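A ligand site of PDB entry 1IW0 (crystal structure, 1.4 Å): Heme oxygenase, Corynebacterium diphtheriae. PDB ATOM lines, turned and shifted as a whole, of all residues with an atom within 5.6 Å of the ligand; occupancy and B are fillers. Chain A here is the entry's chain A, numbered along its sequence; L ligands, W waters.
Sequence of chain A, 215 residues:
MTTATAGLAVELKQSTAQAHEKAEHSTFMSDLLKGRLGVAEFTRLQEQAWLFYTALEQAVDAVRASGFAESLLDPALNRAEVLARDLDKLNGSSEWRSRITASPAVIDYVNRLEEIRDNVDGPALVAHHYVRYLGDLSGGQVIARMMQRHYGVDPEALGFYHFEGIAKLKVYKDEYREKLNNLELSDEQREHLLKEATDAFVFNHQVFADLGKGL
A ring nitrogen (ND1) of His 20 sits at hydrogen-bond distance from the side-chain carboxylate (OE1) of Glu 24.
The side-chain hydroxyl of Tyr 130 sits close to the backbone NH of Lys 13 (3.5 Å).
The side-chain amide oxygen (OD1) of Asn 204 lies within hydrogen-bond range of the guanidinium group (NH1) of Arg 132.
OG of Ser 138 lies within hydrogen-bond range of O of Leu 134 (2.7 Å).
Merely in contact with the ligand: Gly 135 (3.2 Å), Val 131 (3.4 Å), Ala 23 (3.5 Å), Phe 208 (3.5 Å), Lys 13 (3.5 Å), Leu 33 (3.5 Å), Val 142 (3.5 Å), Phe 201 (3.6 Å), Asn 204 (3.6 Å), Gly 139 (3.7 Å), Ser 138 (3.8 Å), Met 29 (3.8 Å) and Leu 134 (3.9 Å).
Of the 23 residues printed, 16 come within 4 Å of the ligand.
The nearest printed residue that does not touch the ligand is Arg 132 (4.1 Å).
Water W5 lies within hydrogen-bond range of O2 of the ligand (2.6 Å), O of Ala 9 (2.9 Å) and NE of Arg 177 (3.0 Å).
Water W2 lies within hydrogen-bond range of an oxygen (O1) of the ligand (2.8 Å) and the guanidinium group (NH2) of Arg 177 (3.2 Å).
A ring nitrogen (NE2) of His 20 binds an iron atom (FE1) of the ligand (2.0 Å).
An oxygen (O2) of the ligand lies within hydrogen-bond range of the side-chain hydroxyl (OH) of Tyr 130, at 2.7 Å.
An oxygen (O1) of the ligand is in salt-bridge range of the guanidinium group (NH2) of Arg 177.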
ATOM      1  N   ALA A   9      -9.047   9.990  29.527  1.00  0.00           N
ATOM      2  CA  ALA A   9      -7.964  10.673  28.805  1.00  0.00           C
ATOM      3  C   ALA A   9      -7.310  11.729  29.682  1.00  0.00           C
ATOM      4  O   ALA A   9      -6.088  11.863  29.708  1.00  0.00           O
ATOM      5  CB  ALA A   9      -8.457  11.257  27.499  1.00  0.00           C
ATOM      6  N   LEU A  12      -5.329   9.955  32.605  1.00  0.00           N
ATOM      7  CA  LEU A  12      -4.074   9.418  32.082  1.00  0.00           C
ATOM      8  C   LEU A  12      -3.015  10.518  31.992  1.00  0.00           C
ATOM      9  O   LEU A  12      -1.897  10.362  32.469  1.00  0.00           O
ATOM     10  CB  LEU A  12      -4.270   8.811  30.697  1.00  0.00           C
ATOM     11  CG  LEU A  12      -4.748   7.354  30.702  1.00  0.00           C
ATOM     12  CD1 LEU A  12      -5.198   6.920  29.343  1.00  0.00           C
ATOM     13  CD2 LEU A  12      -3.663   6.455  31.224  1.00  0.00           C
ATOM     14  N   LYS A  13      -3.378  11.636  31.375  1.00  0.00           N
ATOM     15  CA  LYS A  13      -2.455  12.737  31.216  1.00  0.00           C
ATOM     16  C   LYS A  13      -2.038  13.283  32.551  1.00  0.00           C
ATOM     17  O   LYS A  13      -0.851  13.494  32.809  1.00  0.00           O
ATOM     18  CB  LYS A  13      -3.057  13.847  30.356  1.00  0.00           C
ATOM     19  CG  LYS A  13      -2.021  14.909  29.938  1.00  0.00           C
ATOM     20  CD  LYS A  13      -2.628  15.880  28.948  1.00  0.00           C
ATOM     21  CE  LYS A  13      -1.565  16.833  28.442  1.00  0.00           C
ATOM     22  NZ  LYS A  13      -1.055  17.645  29.581  1.00  0.00           N
ATOM     23  N   HIS A  20       6.260  12.352  32.578  1.00  0.00           N
ATOM     24  CA  HIS A  20       6.608  12.904  31.278  1.00  0.00           C
ATOM     25  C   HIS A  20       7.688  13.980  31.442  1.00  0.00           C
ATOM     26  O   HIS A  20       8.657  14.007  30.685  1.00  0.00           O
ATOM     27  CB  HIS A  20       5.396  13.442  30.538  1.00  0.00           C
ATOM     28  CG  HIS A  20       5.679  13.763  29.102  1.00  0.00           C
ATOM     29  ND1 HIS A  20       6.427  14.856  28.700  1.00  0.00           N
ATOM     30  CD2 HIS A  20       5.354  13.105  27.965  1.00  0.00           C
ATOM     31  CE1 HIS A  20       6.530  14.862  27.383  1.00  0.00           C
ATOM     32  NE2 HIS A  20       5.883  13.812  26.907  1.00  0.00           N
ATOM     33  N   ALA A  23      10.899  12.406  31.867  1.00  0.00           N
ATOM     34  CA  ALA A  23      11.411  11.832  30.625  1.00  0.00           C
ATOM     35  C   ALA A  23      12.111  12.911  29.816  1.00  0.00           C
ATOM     36  O   ALA A  23      13.203  12.692  29.283  1.00  0.00           O
ATOM     37  CB  ALA A  23      10.291  11.196  29.826  1.00  0.00           C
ATOM     38  N   GLU A  24      11.457  14.057  29.709  1.00  0.00           N
ATOM     39  CA  GLU A  24      12.037  15.231  29.039  1.00  0.00           C
ATOM     40  C   GLU A  24      13.401  15.567  29.573  1.00  0.00           C
ATOM     41  O   GLU A  24      14.313  15.938  28.819  1.00  0.00           O
ATOM     42  CB  GLU A  24      11.138  16.451  29.253  1.00  0.00           C
ATOM     43  CG  GLU A  24       9.863  16.451  28.431  1.00  0.00           C
ATOM     44  CD  GLU A  24       8.903  17.520  28.908  1.00  0.00           C
ATOM     45  OE1 GLU A  24       7.864  17.164  29.511  1.00  0.00           O
ATOM     46  OE2 GLU A  24       9.209  18.717  28.698  1.00  0.00           O
ATOM     47  N   MET A  29      18.057  11.688  26.651  1.00  0.00           N
ATOM     48  CA  MET A  29      17.119  12.265  25.701  1.00  0.00           C
ATOM     49  C   MET A  29      17.295  13.784  25.606  1.00  0.00           C
ATOM     50  O   MET A  29      17.161  14.350  24.522  1.00  0.00           O
ATOM     51  CB  MET A  29      15.676  11.879  26.072  1.00  0.00           C
ATOM     52  CG  MET A  29      14.727  12.037  24.918  1.00  0.00           C
ATOM     53  SD  MET A  29      15.182  11.087  23.434  1.00  0.00           S
ATOM     54  CE  MET A  29      13.835  11.537  22.367  1.00  0.00           C
ATOM     55  N   LEU A  33      18.179  15.741  22.166  1.00  0.00           N
ATOM     56  CA  LEU A  33      17.337  16.787  21.599  1.00  0.00           C
ATOM     57  C   LEU A  33      17.976  18.168  21.529  1.00  0.00           C
ATOM     58  O   LEU A  33      17.533  18.967  20.724  1.00  0.00           O
ATOM     59  CB  LEU A  33      16.021  16.889  22.358  1.00  0.00           C
ATOM     60  CG  LEU A  33      15.113  15.664  22.233  1.00  0.00           C
ATOM     61  CD1 LEU A  33      13.834  15.920  22.996  1.00  0.00           C
ATOM     62  CD2 LEU A  33      14.844  15.256  20.815  1.00  0.00           C
ATOM     63  N   TYR A 130      -1.394   4.055  24.705  1.00  0.00           N
ATOM     64  CA  TYR A 130      -1.493   5.471  24.965  1.00  0.00           C
ATOM     65  C   TYR A 130      -0.089   6.033  25.161  1.00  0.00           C
ATOM     66  O   TYR A 130       0.312   7.002  24.488  1.00  0.00           O
ATOM     67  CB  TYR A 130      -2.345   5.709  26.229  1.00  0.00           C
ATOM     68  CG  TYR A 130      -2.106   7.064  26.890  1.00  0.00           C
ATOM     69  CD1 TYR A 130      -2.727   8.204  26.419  1.00  0.00           C
ATOM     70  CD2 TYR A 130      -1.248   7.182  27.961  1.00  0.00           C
ATOM     71  CE1 TYR A 130      -2.502   9.422  27.013  1.00  0.00           C
ATOM     72  CE2 TYR A 130      -1.004   8.418  28.567  1.00  0.00           C
ATOM     73  CZ  TYR A 130      -1.644   9.531  28.081  1.00  0.00           C
ATOM     74  OH  TYR A 130      -1.427  10.788  28.617  1.00  0.00           O
ATOM     75  N   VAL A 131       0.713   5.410  26.026  1.00  0.00           N
ATOM     76  CA  VAL A 131       2.018   5.954  26.390  1.00  0.00           C
ATOM     77  C   VAL A 131       2.923   6.083  25.155  1.00  0.00           C
ATOM     78  O   VAL A 131       3.602   7.101  24.971  1.00  0.00           O
ATOM     79  CB  VAL A 131       2.671   5.167  27.529  1.00  0.00           C
ATOM     80  CG1 VAL A 131       4.111   5.601  27.733  1.00  0.00           C
ATOM     81  CG2 VAL A 131       1.900   5.403  28.832  1.00  0.00           C
ATOM     82  N   ARG A 132       2.924   5.076  24.296  1.00  0.00           N
ATOM     83  CA  ARG A 132       3.720   5.148  23.082  1.00  0.00           C
ATOM     84  C   ARG A 132       3.062   5.929  21.928  1.00  0.00           C
ATOM     85  O   ARG A 132       3.591   6.950  21.493  1.00  0.00           O
ATOM     86  CB  ARG A 132       4.166   3.750  22.609  1.00  0.00           C
ATOM     87  CG  ARG A 132       5.275   3.161  23.451  1.00  0.00           C
ATOM     88  CD  ARG A 132       6.496   4.006  23.720  1.00  0.00           C
ATOM     89  NE  ARG A 132       6.904   4.830  22.587  1.00  0.00           N
ATOM     90  CZ  ARG A 132       7.880   5.719  22.649  1.00  0.00           C
ATOM     91  NH1 ARG A 132       8.597   5.874  23.745  1.00  0.00           N
ATOM     92  NH2 ARG A 132       8.163   6.482  21.586  1.00  0.00           N
ATOM     93  N   LEU A 134       0.167   7.782  21.501  1.00  0.00           N
ATOM     94  CA  LEU A 134      -0.311   9.162  21.615  1.00  0.00           C
ATOM     95  C   LEU A 134       0.902  10.063  21.765  1.00  0.00           C
ATOM     96  O   LEU A 134       0.873  11.206  21.297  1.00  0.00           O
ATOM     97  CB  LEU A 134      -1.292   9.378  22.748  1.00  0.00           C
ATOM     98  CG  LEU A 134      -2.045  10.709  22.584  1.00  0.00           C
ATOM     99  CD1 LEU A 134      -2.701  10.885  21.253  1.00  0.00           C
ATOM    100  CD2 LEU A 134      -3.043  10.843  23.643  1.00  0.00           C
ATOM    101  N   GLY A 135       1.945   9.601  22.433  1.00  0.00           N
ATOM    102  CA  GLY A 135       3.160  10.390  22.539  1.00  0.00           C
ATOM    103  C   GLY A 135       3.779  10.623  21.176  1.00  0.00           C
ATOM    104  O   GLY A 135       4.233  11.731  20.872  1.00  0.00           O
ATOM    105  N   ASP A 136       3.840   9.594  20.355  1.00  0.00           N
ATOM    106  CA  ASP A 136       4.426   9.724  19.026  1.00  0.00           C
ATOM    107  C   ASP A 136       3.629  10.709  18.171  1.00  0.00           C
ATOM    108  O   ASP A 136       4.207  11.494  17.408  1.00  0.00           O
ATOM    109  CB  ASP A 136       4.415   8.380  18.285  1.00  0.00           C
ATOM    110  CG  ASP A 136       5.221   7.305  18.985  1.00  0.00           C
ATOM    111  OD1 ASP A 136       4.856   6.130  18.740  1.00  0.00           O
ATOM    112  OD2 ASP A 136       6.185   7.556  19.714  1.00  0.00           O
ATOM    113  N   SER A 138       1.599  13.061  19.182  1.00  0.00           N
ATOM    114  CA  SER A 138       1.467  14.362  19.794  1.00  0.00           C
ATOM    115  C   SER A 138       2.749  15.161  19.828  1.00  0.00           C
ATOM    116  O   SER A 138       2.711  16.354  19.471  1.00  0.00           O
ATOM    117  CB  SER A 138       0.865  14.220  21.201  1.00  0.00           C
ATOM    118  OG  SER A 138      -0.384  13.544  21.137  1.00  0.00           O
ATOM    119  N   GLY A 139       3.858  14.544  20.243  1.00  0.00           N
ATOM    120  CA  GLY A 139       5.146  15.191  20.400  1.00  0.00           C
ATOM    121  C   GLY A 139       6.237  14.680  19.450  1.00  0.00           C
ATOM    122  O   GLY A 139       7.351  15.198  19.419  1.00  0.00           O
ATOM    123  N   VAL A 142       8.116  17.131  17.110  1.00  0.00           N
ATOM    124  CA  VAL A 142       9.186  17.916  17.725  1.00  0.00           C
ATOM    125  C   VAL A 142      10.507  17.137  17.694  1.00  0.00           C
ATOM    126  O   VAL A 142      11.578  17.660  17.406  1.00  0.00           O
ATOM    127  CB  VAL A 142       8.831  18.313  19.170  1.00  0.00           C
ATOM    128  CG1 VAL A 142      10.055  18.878  19.919  1.00  0.00           C
ATOM    129  CG2 VAL A 142       7.655  19.284  19.144  1.00  0.00           C
ATOM    130  N   ILE A 143      10.433  15.865  18.043  1.00  0.00           N
ATOM    131  CA  ILE A 143      11.614  15.029  18.033  1.00  0.00           C
ATOM    132  C   ILE A 143      12.166  14.919  16.600  1.00  0.00           C
ATOM    133  O   ILE A 143      13.368  15.058  16.400  1.00  0.00           O
ATOM    134  CB  ILE A 143      11.294  13.640  18.644  1.00  0.00           C
ATOM    135  CG1 ILE A 143      10.929  13.784  20.133  1.00  0.00           C
ATOM    136  CG2 ILE A 143      12.497  12.765  18.521  1.00  0.00           C
ATOM    137  CD1 ILE A 143      10.332  12.508  20.755  1.00  0.00           C
ATOM    138  N   ARG A 177      -8.530  10.332  22.007  1.00  0.00           N
ATOM    139  CA  ARG A 177      -8.961  10.641  23.365  1.00  0.00           C
ATOM    140  C   ARG A 177     -10.444  10.292  23.612  1.00  0.00           C
ATOM    141  O   ARG A 177     -10.787   9.768  24.680  1.00  0.00           O
ATOM    142  CB  ARG A 177      -8.656  12.085  23.724  1.00  0.00           C
ATOM    143  CG  ARG A 177      -7.202  12.341  23.892  1.00  0.00           C
ATOM    144  CD  ARG A 177      -6.899  13.685  24.485  1.00  0.00           C
ATOM    145  NE  ARG A 177      -5.478  13.973  24.407  1.00  0.00           N
ATOM    146  CZ  ARG A 177      -4.878  14.563  23.385  1.00  0.00           C
ATOM    147  NH1 ARG A 177      -5.581  14.978  22.340  1.00  0.00           N
ATOM    148  NH2 ARG A 177      -3.569  14.764  23.396  1.00  0.00           N
ATOM    149  N   PHE A 201       5.695   4.493  31.481  1.00  0.00           N
ATOM    150  CA  PHE A 201       6.642   5.601  31.542  1.00  0.00           C
ATOM    151  C   PHE A 201       7.954   5.178  32.208  1.00  0.00           C
ATOM    152  O   PHE A 201       9.059   5.519  31.757  1.00  0.00           O
ATOM    153  CB  PHE A 201       6.067   6.833  32.227  1.00  0.00           C
ATOM    154  CG  PHE A 201       5.415   7.794  31.273  1.00  0.00           C
ATOM    155  CD1 PHE A 201       4.073   7.756  31.000  1.00  0.00           C
ATOM    156  CD2 PHE A 201       6.192   8.727  30.603  1.00  0.00           C
ATOM    157  CE1 PHE A 201       3.493   8.630  30.090  1.00  0.00           C
ATOM    158  CE2 PHE A 201       5.637   9.595  29.711  1.00  0.00           C
ATOM    159  CZ  PHE A 201       4.303   9.565  29.444  1.00  0.00           C
ATOM    160  N   ASN A 204      10.085   3.280  29.779  1.00  0.00           N
ATOM    161  CA  ASN A 204      10.623   4.184  28.760  1.00  0.00           C
ATOM    162  C   ASN A 204      11.742   5.085  29.296  1.00  0.00           C
ATOM    163  O   ASN A 204      12.736   5.305  28.626  1.00  0.00           O
ATOM    164  CB  ASN A 204       9.505   4.976  28.108  1.00  0.00           C
ATOM    165  CG  ASN A 204       8.857   4.212  26.988  1.00  0.00           C
ATOM    166  OD1 ASN A 204       9.360   4.160  25.885  1.00  0.00           O
ATOM    167  ND2 ASN A 204       7.714   3.581  27.295  1.00  0.00           N
ATOM    168  N   HIS A 205      11.589   5.570  30.508  1.00  0.00           N
ATOM    169  CA  HIS A 205      12.680   6.327  31.112  1.00  0.00           C
ATOM    170  C   HIS A 205      13.945   5.474  31.260  1.00  0.00           C
ATOM    171  O   HIS A 205      15.076   5.927  30.994  1.00  0.00           O
ATOM    172  CB  HIS A 205      12.274   6.846  32.464  1.00  0.00           C
ATOM    173  CG  HIS A 205      13.352   7.640  33.119  1.00  0.00           C
ATOM    174  ND1 HIS A 205      14.355   7.049  33.867  1.00  0.00           N
ATOM    175  CD2 HIS A 205      13.621   8.958  33.096  1.00  0.00           C
ATOM    176  CE1 HIS A 205      15.191   7.991  34.279  1.00  0.00           C
ATOM    177  NE2 HIS A 205      14.754   9.161  33.839  1.00  0.00           N
ATOM    178  N   PHE A 208      16.051   5.152  28.205  1.00  0.00           N
ATOM    179  CA  PHE A 208      16.912   6.321  28.032  1.00  0.00           C
ATOM    180  C   PHE A 208      18.116   6.213  28.973  1.00  0.00           C
ATOM    181  O   PHE A 208      19.251   6.497  28.571  1.00  0.00           O
ATOM    182  CB  PHE A 208      16.174   7.592  28.417  1.00  0.00           C
ATOM    183  CG  PHE A 208      15.073   8.016  27.463  1.00  0.00           C
ATOM    184  CD1 PHE A 208      15.044   7.614  26.155  1.00  0.00           C
ATOM    185  CD2 PHE A 208      14.083   8.868  27.899  1.00  0.00           C
ATOM    186  CE1 PHE A 208      14.034   8.035  25.309  1.00  0.00           C
ATOM    187  CE2 PHE A 208      13.085   9.319  27.056  1.00  0.00           C
ATOM    188  CZ  PHE A 208      13.046   8.890  25.769  1.00  0.00           C
HETATM  189  C1  LIG L   1       2.740  14.357  24.473  1.00  0.00           C
HETATM  190  C2  LIG L   1       4.726  10.173  25.960  1.00  0.00           C
HETATM  191  C3  LIG L   1       9.085  12.116  25.540  1.00  0.00           C
HETATM  192  C4  LIG L   1       7.295  16.156  23.827  1.00  0.00           C
HETATM  193  C5  LIG L   1       2.943  13.030  24.960  1.00  0.00           C
HETATM  194  C6  LIG L   1       1.771  12.277  25.254  1.00  0.00           C
HETATM  195  C7  LIG L   1       2.331  11.140  25.649  1.00  0.00           C
HETATM  196  C8  LIG L   1       3.818  11.138  25.631  1.00  0.00           C
HETATM  197  C9  LIG L   1       1.669   9.880  26.121  1.00  0.00           C
HETATM  198  C10 LIG L   1       0.276  12.581  25.171  1.00  0.00           C
HETATM  199  C11 LIG L   1      -0.149  13.317  26.426  1.00  0.00           C
HETATM  200  C12 LIG L   1      -1.626  13.485  26.375  1.00  0.00           C
HETATM  201  O1  LIG L   1      -2.049  14.340  25.593  1.00  0.00           O
HETATM  202  O2  LIG L   1      -2.387  12.756  27.099  1.00  0.00           O
HETATM  203  C13 LIG L   1       6.053  10.295  25.954  1.00  0.00           C
HETATM  204  C14 LIG L   1       7.062   9.326  26.329  1.00  0.00           C
HETATM  205  C15 LIG L   1       8.253   9.891  26.206  1.00  0.00           C
HETATM  206  C16 LIG L   1       8.022  11.270  25.758  1.00  0.00           C
HETATM  207  C17 LIG L   1       6.635   7.904  26.738  1.00  0.00           C
HETATM  208  C18 LIG L   1       9.566   9.160  26.506  1.00  0.00           C
HETATM  209  C19 LIG L   1       9.746   8.524  27.685  1.00  0.00           C
HETATM  210  C20 LIG L   1       8.916  13.379  25.057  1.00  0.00           C
HETATM  211  C21 LIG L   1      10.055  14.264  24.845  1.00  0.00           C
HETATM  212  C22 LIG L   1       9.526  15.362  24.372  1.00  0.00           C
HETATM  213  C23 LIG L   1       8.130  15.224  24.260  1.00  0.00           C
HETATM  214  C24 LIG L   1      11.436  13.894  25.155  1.00  0.00           C
HETATM  215  C25 LIG L   1      10.508  16.483  24.074  1.00  0.00           C
HETATM  216  C26 LIG L   1      10.348  16.938  22.871  1.00  0.00           C
HETATM  217  C27 LIG L   1       5.927  16.075  23.874  1.00  0.00           C
HETATM  218  C28 LIG L   1       4.947  17.080  23.553  1.00  0.00           C
HETATM  219  C29 LIG L   1       3.566  16.575  23.725  1.00  0.00           C
HETATM  220  C30 LIG L   1       3.806  15.138  24.193  1.00  0.00           C
HETATM  221  C31 LIG L   1       5.343  18.520  23.084  1.00  0.00           C
HETATM  222  C32 LIG L   1       2.366  17.491  23.432  1.00  0.00           C
HETATM  223  C33 LIG L   1       1.996  18.069  24.726  1.00  0.00           C
HETATM  224  C34 LIG L   1       2.571  17.972  26.006  1.00  0.00           C
HETATM  225  O3  LIG L   1       2.493  17.370  27.080  1.00  0.00           O
HETATM  226  O4  LIG L   1       3.456  18.787  25.969  1.00  0.00           O
HETATM  227  N1  LIG L   1       4.133  12.432  25.166  1.00  0.00           N
HETATM  228  N2  LIG L   1       6.751  11.449  25.629  1.00  0.00           N
HETATM  229  N3  LIG L   1       7.831  13.944  24.713  1.00  0.00           N
HETATM  230  N4  LIG L   1       5.191  14.937  24.289  1.00  0.00           N
HETATM  231 FE1  LIG L   1       5.979  13.224  24.993  1.00  0.00          FE
HETATM  232  O   HOH W   1       7.528  10.015  22.641  1.00  0.00           O
HETATM  233  O   HOH W   2      -3.765  16.504  26.066  1.00  0.00           O
HETATM  234  O   HOH W   3       6.200  12.501  23.040  1.00  0.00           O
HETATM  235  O   HOH W   4      -0.618  16.295  24.654  1.00  0.00           O
HETATM  236  O   HOH W   5      -4.979  12.888  27.178  1.00  0.00           O
